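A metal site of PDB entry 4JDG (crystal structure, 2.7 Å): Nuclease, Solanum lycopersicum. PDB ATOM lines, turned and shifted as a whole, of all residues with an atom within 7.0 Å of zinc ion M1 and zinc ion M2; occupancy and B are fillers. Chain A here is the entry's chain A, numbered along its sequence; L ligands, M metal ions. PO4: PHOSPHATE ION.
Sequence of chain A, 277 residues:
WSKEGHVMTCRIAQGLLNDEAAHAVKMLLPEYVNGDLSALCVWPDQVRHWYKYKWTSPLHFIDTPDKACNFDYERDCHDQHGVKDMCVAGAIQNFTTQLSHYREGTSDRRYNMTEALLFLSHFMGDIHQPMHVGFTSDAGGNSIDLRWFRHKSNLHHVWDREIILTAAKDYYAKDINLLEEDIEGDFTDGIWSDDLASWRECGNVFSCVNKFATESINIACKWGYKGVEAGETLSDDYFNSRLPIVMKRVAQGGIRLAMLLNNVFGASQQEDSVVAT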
ATOM      1  N   TRP A   1      16.879 -18.569 -19.639  1.00  0.00           N
ATOM      2  CA  TRP A   1      16.317 -17.605 -20.592  1.00  0.00           C
ATOM      3  C   TRP A   1      16.626 -18.045 -22.019  1.00  0.00           C
ATOM      4  O   TRP A   1      17.600 -18.742 -22.256  1.00  0.00           O
ATOM      5  CB  TRP A   1      16.937 -16.237 -20.377  1.00  0.00           C
ATOM      6  CG  TRP A   1      16.736 -15.562 -19.018  1.00  0.00           C
ATOM      7  CD1 TRP A   1      17.729 -15.118 -18.190  1.00  0.00           C
ATOM      8  CD2 TRP A   1      15.501 -15.191 -18.391  1.00  0.00           C
ATOM      9  NE1 TRP A   1      17.199 -14.517 -17.088  1.00  0.00           N
ATOM     10  CE2 TRP A   1      15.830 -14.543 -17.183  1.00  0.00           C
ATOM     11  CE3 TRP A   1      14.156 -15.338 -18.732  1.00  0.00           C
ATOM     12  CZ2 TRP A   1      14.857 -14.056 -16.308  1.00  0.00           C
ATOM     13  CZ3 TRP A   1      13.190 -14.845 -17.857  1.00  0.00           C
ATOM     14  CH2 TRP A   1      13.546 -14.224 -16.662  1.00  0.00           C
ATOM     15  N   SER A   2      15.791 -17.618 -22.972  1.00  0.00           N
ATOM     16  CA  SER A   2      16.069 -17.769 -24.382  1.00  0.00           C
ATOM     17  C   SER A   2      16.871 -16.564 -24.802  1.00  0.00           C
ATOM     18  O   SER A   2      17.223 -15.749 -23.955  1.00  0.00           O
ATOM     19  CB  SER A   2      14.781 -17.868 -25.155  1.00  0.00           C
ATOM     20  OG  SER A   2      14.037 -18.961 -24.648  1.00  0.00           O
ATOM     21  N   LYS A   3      17.152 -16.448 -26.098  1.00  0.00           N
ATOM     22  CA  LYS A   3      17.996 -15.358 -26.603  1.00  0.00           C
ATOM     23  C   LYS A   3      17.795 -14.087 -25.809  1.00  0.00           C
ATOM     24  O   LYS A   3      18.753 -13.501 -25.267  1.00  0.00           O
ATOM     25  CB  LYS A   3      17.686 -15.061 -28.077  1.00  0.00           C
ATOM     26  CG  LYS A   3      17.896 -16.253 -29.005  1.00  0.00           C
ATOM     27  CD  LYS A   3      18.734 -15.863 -30.218  1.00  0.00           C
ATOM     28  CE  LYS A   3      19.580 -17.027 -30.688  1.00  0.00           C
ATOM     29  NZ  LYS A   3      20.591 -16.675 -31.710  1.00  0.00           N
ATOM     30  N   GLY A   5      16.304 -12.926 -22.850  1.00  0.00           N
ATOM     31  CA  GLY A   5      16.698 -12.749 -21.440  1.00  0.00           C
ATOM     32  C   GLY A   5      18.202 -12.633 -21.279  1.00  0.00           C
ATOM     33  O   GLY A   5      18.715 -11.707 -20.619  1.00  0.00           O
ATOM     34  N   HIS A   6      18.927 -13.542 -21.922  1.00  0.00           N
ATOM     35  CA  HIS A   6      20.373 -13.481 -21.856  1.00  0.00           C
ATOM     36  C   HIS A   6      20.932 -12.182 -22.422  1.00  0.00           C
ATOM     37  O   HIS A   6      21.809 -11.573 -21.810  1.00  0.00           O
ATOM     38  CB  HIS A   6      20.982 -14.685 -22.538  1.00  0.00           C
ATOM     39  CG  HIS A   6      20.677 -15.959 -21.835  1.00  0.00           C
ATOM     40  ND1 HIS A   6      21.231 -16.274 -20.610  1.00  0.00           N
ATOM     41  CD2 HIS A   6      19.855 -16.989 -22.145  1.00  0.00           C
ATOM     42  CE1 HIS A   6      20.756 -17.441 -20.209  1.00  0.00           C
ATOM     43  NE2 HIS A   6      19.939 -17.893 -21.132  1.00  0.00           N
ATOM     44  N   CYS A  41      26.295 -14.471 -25.295  1.00  0.00           N
ATOM     45  CA  CYS A  41      25.706 -15.059 -24.072  1.00  0.00           C
ATOM     46  C   CYS A  41      24.838 -16.286 -24.324  1.00  0.00           C
ATOM     47  O   CYS A  41      24.580 -17.038 -23.408  1.00  0.00           O
ATOM     48  CB  CYS A  41      24.922 -14.006 -23.264  1.00  0.00           C
ATOM     49  SG  CYS A  41      26.072 -12.921 -22.383  1.00  0.00           S
ATOM     50  N   VAL A  42      24.355 -16.474 -25.544  1.00  0.00           N
ATOM     51  CA  VAL A  42      23.543 -17.657 -25.859  1.00  0.00           C
ATOM     52  C   VAL A  42      24.445 -18.852 -26.179  1.00  0.00           C
ATOM     53  O   VAL A  42      24.025 -19.986 -26.086  1.00  0.00           O
ATOM     54  CB  VAL A  42      22.549 -17.365 -27.020  1.00  0.00           C
ATOM     55  CG1 VAL A  42      21.713 -18.580 -27.363  1.00  0.00           C
ATOM     56  CG2 VAL A  42      21.612 -16.264 -26.598  1.00  0.00           C
ATOM     57  N   PRO A  44      26.417 -20.941 -24.905  1.00  0.00           N
ATOM     58  CA  PRO A  44      26.279 -22.215 -24.205  1.00  0.00           C
ATOM     59  C   PRO A  44      25.043 -23.005 -24.564  1.00  0.00           C
ATOM     60  O   PRO A  44      24.983 -24.195 -24.276  1.00  0.00           O
ATOM     61  CB  PRO A  44      26.203 -21.800 -22.737  1.00  0.00           C
ATOM     62  CG  PRO A  44      26.967 -20.534 -22.695  1.00  0.00           C
ATOM     63  CD  PRO A  44      26.632 -19.828 -23.965  1.00  0.00           C
ATOM     64  N   ASP A  45      24.043 -22.341 -25.130  1.00  0.00           N
ATOM     65  CA  ASP A  45      22.754 -22.977 -25.405  1.00  0.00           C
ATOM     66  C   ASP A  45      22.813 -23.692 -26.744  1.00  0.00           C
ATOM     67  O   ASP A  45      22.013 -24.587 -27.013  1.00  0.00           O
ATOM     68  CB  ASP A  45      21.631 -21.922 -25.446  1.00  0.00           C
ATOM     69  CG  ASP A  45      20.664 -22.020 -24.289  1.00  0.00           C
ATOM     70  OD1 ASP A  45      20.576 -23.059 -23.608  1.00  0.00           O
ATOM     71  OD2 ASP A  45      19.919 -21.042 -24.094  1.00  0.00           O
ATOM     72  N   ARG A  48      25.161 -26.877 -26.046  1.00  0.00           N
ATOM     73  CA  ARG A  48      24.373 -27.771 -25.200  1.00  0.00           C
ATOM     74  C   ARG A  48      24.084 -29.128 -25.877  1.00  0.00           C
ATOM     75  O   ARG A  48      23.918 -30.144 -25.198  1.00  0.00           O
ATOM     76  CB  ARG A  48      23.053 -27.021 -24.916  1.00  0.00           C
ATOM     77  CG  ARG A  48      22.064 -27.639 -23.946  1.00  0.00           C
ATOM     78  CD  ARG A  48      20.781 -26.793 -23.932  1.00  0.00           C
ATOM     79  NE  ARG A  48      20.296 -26.500 -22.590  1.00  0.00           N
ATOM     80  CZ  ARG A  48      19.835 -27.415 -21.732  1.00  0.00           C
ATOM     81  NH1 ARG A  48      19.826 -28.707 -22.050  1.00  0.00           N
ATOM     82  NH2 ARG A  48      19.401 -27.044 -20.531  1.00  0.00           N
ATOM     83  N   LEU A  59      24.065 -28.386 -16.313  1.00  0.00           N
ATOM     84  CA  LEU A  59      24.539 -27.146 -15.690  1.00  0.00           C
ATOM     85  C   LEU A  59      23.621 -25.955 -15.936  1.00  0.00           C
ATOM     86  O   LEU A  59      23.957 -24.828 -15.579  1.00  0.00           O
ATOM     87  CB  LEU A  59      25.964 -26.796 -16.205  1.00  0.00           C
ATOM     88  CG  LEU A  59      27.131 -27.770 -16.038  1.00  0.00           C
ATOM     89  CD1 LEU A  59      28.452 -27.128 -16.453  1.00  0.00           C
ATOM     90  CD2 LEU A  59      27.232 -28.209 -14.598  1.00  0.00           C
ATOM     91  N   HIS A  60      22.499 -26.141 -16.598  1.00  0.00           N
ATOM     92  CA  HIS A  60      21.634 -24.989 -16.910  1.00  0.00           C
ATOM     93  C   HIS A  60      20.584 -24.770 -15.841  1.00  0.00           C
ATOM     94  O   HIS A  60      20.023 -23.665 -15.715  1.00  0.00           O
ATOM     95  CB  HIS A  60      20.964 -25.198 -18.272  1.00  0.00           C
ATOM     96  CG  HIS A  60      21.908 -24.976 -19.408  1.00  0.00           C
ATOM     97  ND1 HIS A  60      21.705 -24.008 -20.363  1.00  0.00           N
ATOM     98  CD2 HIS A  60      23.077 -25.571 -19.730  1.00  0.00           C
ATOM     99  CE1 HIS A  60      22.712 -24.012 -21.217  1.00  0.00           C
ATOM    100  NE2 HIS A  60      23.550 -24.966 -20.858  1.00  0.00           N
ATOM    101  N   PHE A  61      20.337 -25.819 -15.046  1.00  0.00           N
ATOM    102  CA  PHE A  61      19.233 -25.830 -14.133  1.00  0.00           C
ATOM    103  C   PHE A  61      19.531 -26.501 -12.794  1.00  0.00           C
ATOM    104  O   PHE A  61      20.673 -26.933 -12.516  1.00  0.00           O
ATOM    105  CB  PHE A  61      18.061 -26.523 -14.808  1.00  0.00           C
ATOM    106  CG  PHE A  61      18.373 -27.899 -15.273  1.00  0.00           C
ATOM    107  CD1 PHE A  61      18.910 -28.117 -16.531  1.00  0.00           C
ATOM    108  CD2 PHE A  61      18.082 -29.002 -14.484  1.00  0.00           C
ATOM    109  CE1 PHE A  61      19.173 -29.414 -16.972  1.00  0.00           C
ATOM    110  CE2 PHE A  61      18.345 -30.299 -14.925  1.00  0.00           C
ATOM    111  CZ  PHE A  61      18.892 -30.499 -16.155  1.00  0.00           C
ATOM    112  N   HIS A 122      26.237 -16.638 -19.049  1.00  0.00           N
ATOM    113  CA  HIS A 122      25.004 -17.330 -19.422  1.00  0.00           C
ATOM    114  C   HIS A 122      24.293 -17.921 -18.218  1.00  0.00           C
ATOM    115  O   HIS A 122      23.100 -17.716 -18.044  1.00  0.00           O
ATOM    116  CB  HIS A 122      25.305 -18.457 -20.396  1.00  0.00           C
ATOM    117  CG  HIS A 122      24.091 -19.212 -20.808  1.00  0.00           C
ATOM    118  ND1 HIS A 122      23.336 -18.849 -21.898  1.00  0.00           N
ATOM    119  CD2 HIS A 122      23.466 -20.269 -20.230  1.00  0.00           C
ATOM    120  CE1 HIS A 122      22.296 -19.673 -21.991  1.00  0.00           C
ATOM    121  NE2 HIS A 122      22.361 -20.542 -21.000  1.00  0.00           N
ATOM    122  N   PHE A 123      25.018 -18.678 -17.407  1.00  0.00           N
ATOM    123  CA  PHE A 123      24.451 -19.346 -16.219  1.00  0.00           C
ATOM    124  C   PHE A 123      24.022 -18.391 -15.103  1.00  0.00           C
ATOM    125  O   PHE A 123      23.145 -18.706 -14.290  1.00  0.00           O
ATOM    126  CB  PHE A 123      25.441 -20.357 -15.670  1.00  0.00           C
ATOM    127  CG  PHE A 123      25.760 -21.489 -16.618  1.00  0.00           C
ATOM    128  CD1 PHE A 123      24.758 -22.245 -17.149  1.00  0.00           C
ATOM    129  CD2 PHE A 123      27.073 -21.831 -16.897  1.00  0.00           C
ATOM    130  CE1 PHE A 123      25.039 -23.296 -18.006  1.00  0.00           C
ATOM    131  CE2 PHE A 123      27.365 -22.879 -17.746  1.00  0.00           C
ATOM    132  CZ  PHE A 123      26.343 -23.613 -18.305  1.00  0.00           C
ATOM    133  N   GLY A 125      22.422 -15.689 -15.765  1.00  0.00           N
ATOM    134  CA  GLY A 125      21.066 -15.422 -16.241  1.00  0.00           C
ATOM    135  C   GLY A 125      20.128 -16.597 -16.020  1.00  0.00           C
ATOM    136  O   GLY A 125      18.955 -16.385 -15.685  1.00  0.00           O
ATOM    137  N   ASP A 126      20.622 -17.834 -16.202  1.00  0.00           N
ATOM    138  CA  ASP A 126      19.744 -19.013 -16.058  1.00  0.00           C
ATOM    139  C   ASP A 126      19.263 -19.199 -14.609  1.00  0.00           C
ATOM    140  O   ASP A 126      18.101 -19.542 -14.387  1.00  0.00           O
ATOM    141  CB  ASP A 126      20.422 -20.306 -16.551  1.00  0.00           C
ATOM    142  CG  ASP A 126      20.128 -20.613 -18.041  1.00  0.00           C
ATOM    143  OD1 ASP A 126      19.544 -19.787 -18.739  1.00  0.00           O
ATOM    144  OD2 ASP A 126      20.503 -21.709 -18.509  1.00  0.00           O
ATOM    145  N   GLN A 129      16.166 -17.188 -13.813  1.00  0.00           N
ATOM    146  CA  GLN A 129      14.928 -17.627 -14.471  1.00  0.00           C
ATOM    147  C   GLN A 129      14.255 -18.584 -13.503  1.00  0.00           C
ATOM    148  O   GLN A 129      14.715 -19.705 -13.353  1.00  0.00           O
ATOM    149  CB  GLN A 129      15.209 -18.327 -15.807  1.00  0.00           C
ATOM    150  CG  GLN A 129      14.103 -18.165 -16.835  1.00  0.00           C
ATOM    151  CD  GLN A 129      12.980 -19.150 -16.657  1.00  0.00           C
ATOM    152  OE1 GLN A 129      12.438 -19.311 -15.576  1.00  0.00           O
ATOM    153  NE2 GLN A 129      12.628 -19.834 -17.740  1.00  0.00           N
ATOM    154  N   HIS A 132      14.134 -22.313 -13.835  1.00  0.00           N
ATOM    155  CA  HIS A 132      15.383 -23.081 -13.881  1.00  0.00           C
ATOM    156  C   HIS A 132      15.714 -23.755 -12.559  1.00  0.00           C
ATOM    157  O   HIS A 132      16.653 -24.550 -12.468  1.00  0.00           O
ATOM    158  CB  HIS A 132      16.536 -22.208 -14.364  1.00  0.00           C
ATOM    159  CG  HIS A 132      16.590 -22.127 -15.850  1.00  0.00           C
ATOM    160  ND1 HIS A 132      17.647 -22.630 -16.579  1.00  0.00           N
ATOM    161  CD2 HIS A 132      15.664 -21.722 -16.749  1.00  0.00           C
ATOM    162  CE1 HIS A 132      17.389 -22.476 -17.857  1.00  0.00           C
ATOM    163  NE2 HIS A 132      16.186 -21.939 -17.988  1.00  0.00           N
ATOM    164  N   ASP A 160      10.844 -18.511 -20.102  1.00  0.00           N
ATOM    165  CA  ASP A 160      12.067 -18.336 -20.919  1.00  0.00           C
ATOM    166  C   ASP A 160      11.885 -17.288 -22.013  1.00  0.00           C
ATOM    167  O   ASP A 160      12.849 -16.638 -22.420  1.00  0.00           O
ATOM    168  CB  ASP A 160      12.475 -19.650 -21.588  1.00  0.00           C
ATOM    169  CG  ASP A 160      13.502 -20.416 -20.808  1.00  0.00           C
ATOM    170  OD1 ASP A 160      14.711 -20.122 -20.944  1.00  0.00           O
ATOM    171  OD2 ASP A 160      13.110 -21.329 -20.063  1.00  0.00           O
HETATM  172  P   PO4 L   1      17.943 -21.834 -21.315  1.00  0.00           P
HETATM  173  O1  PO4 L   1      17.227 -20.882 -20.323  1.00  0.00           O
HETATM  174  O2  PO4 L   1      16.899 -22.496 -22.235  1.00  0.00           O
HETATM  175  O3  PO4 L   1      18.908 -20.992 -22.133  1.00  0.00           O
HETATM  176  O4  PO4 L   1      18.810 -22.921 -20.650  1.00  0.00           O
HETATM  177 ZN    ZN M   1      20.812 -22.010 -20.658  1.00  0.00          ZN
HETATM  178 ZN    ZN M   2      18.791 -19.302 -20.642  1.00  0.00          ZN
HETATM  179 ZN    ZN M   3      15.178 -22.422 -20.078  1.00  0.00          ZN
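Zinc ion M2 is bound by a ring nitrogen (NE2) of His 6 (1.9 Å), the backbone carbonyl oxygen of Trp 1 (2.1 Å), the side-chain carboxylate of Asp 126 (2.1 Å), an oxygen (O1) of the ligand (2.2 Å), an oxygen (O3) of the ligand (2.3 Å) and the backbone nitrogen of Trp 1 (2.3 Å). Zinc ion M2 has six donor atoms within binding distance.
Of the 20 residues printed, 4 come within 4 Å of zinc ion M2. The nearest printed residue that does not touch zinc ion M2 is Asp 45 (4.03 Å).
NE2 of His 122 binds zinc ion M1, at 2.2 Å. Zinc ion M1 is bound by OD2 of Asp 126 (2.2 Å). Zinc ion M1 is bound by O4 of the ligand (2.2 Å). ND1 of His 60 binds zinc ion M1, 2.2 Å away. Slightly farther from zinc ion M1 lies an oxygen (O3) of the ligand (2.6 Å).
A ring nitrogen (ND1) of His 6 lies close to the backbone carbonyl oxygen of His 122, 3.5 Å away. The indole nitrogen (NE1) of Trp 1 lies within hydrogen-bond range of the backbone carbonyl oxygen (O) of Gly 125 (2.9 Å). The backbone carbonyl oxygen of Cys 41 is in hydrogen-bond range of a ring nitrogen (ND1) of His 122, at 2.7 Å. The backbone carbonyl oxygen (O) of His 60 sits at hydrogen-bond distance from a ring nitrogen (ND1) of His 132 (2.7 Å). The guanidinium group of Arg 48 lies within salt-bridge range of the side-chain carboxylate of Asp 45 (3.6 Å).
OD1 of Asp 45 touches zinc ion M1 (3.1 Å). Of the 20 residues printed, 4 come within 4 Å of zinc ion M1. Along chain A the residues within 4 Å of zinc ion M1 span positions 45 to 126. The nearest printed residue that does not touch zinc ion M1 is His 6 (4.2 Å).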
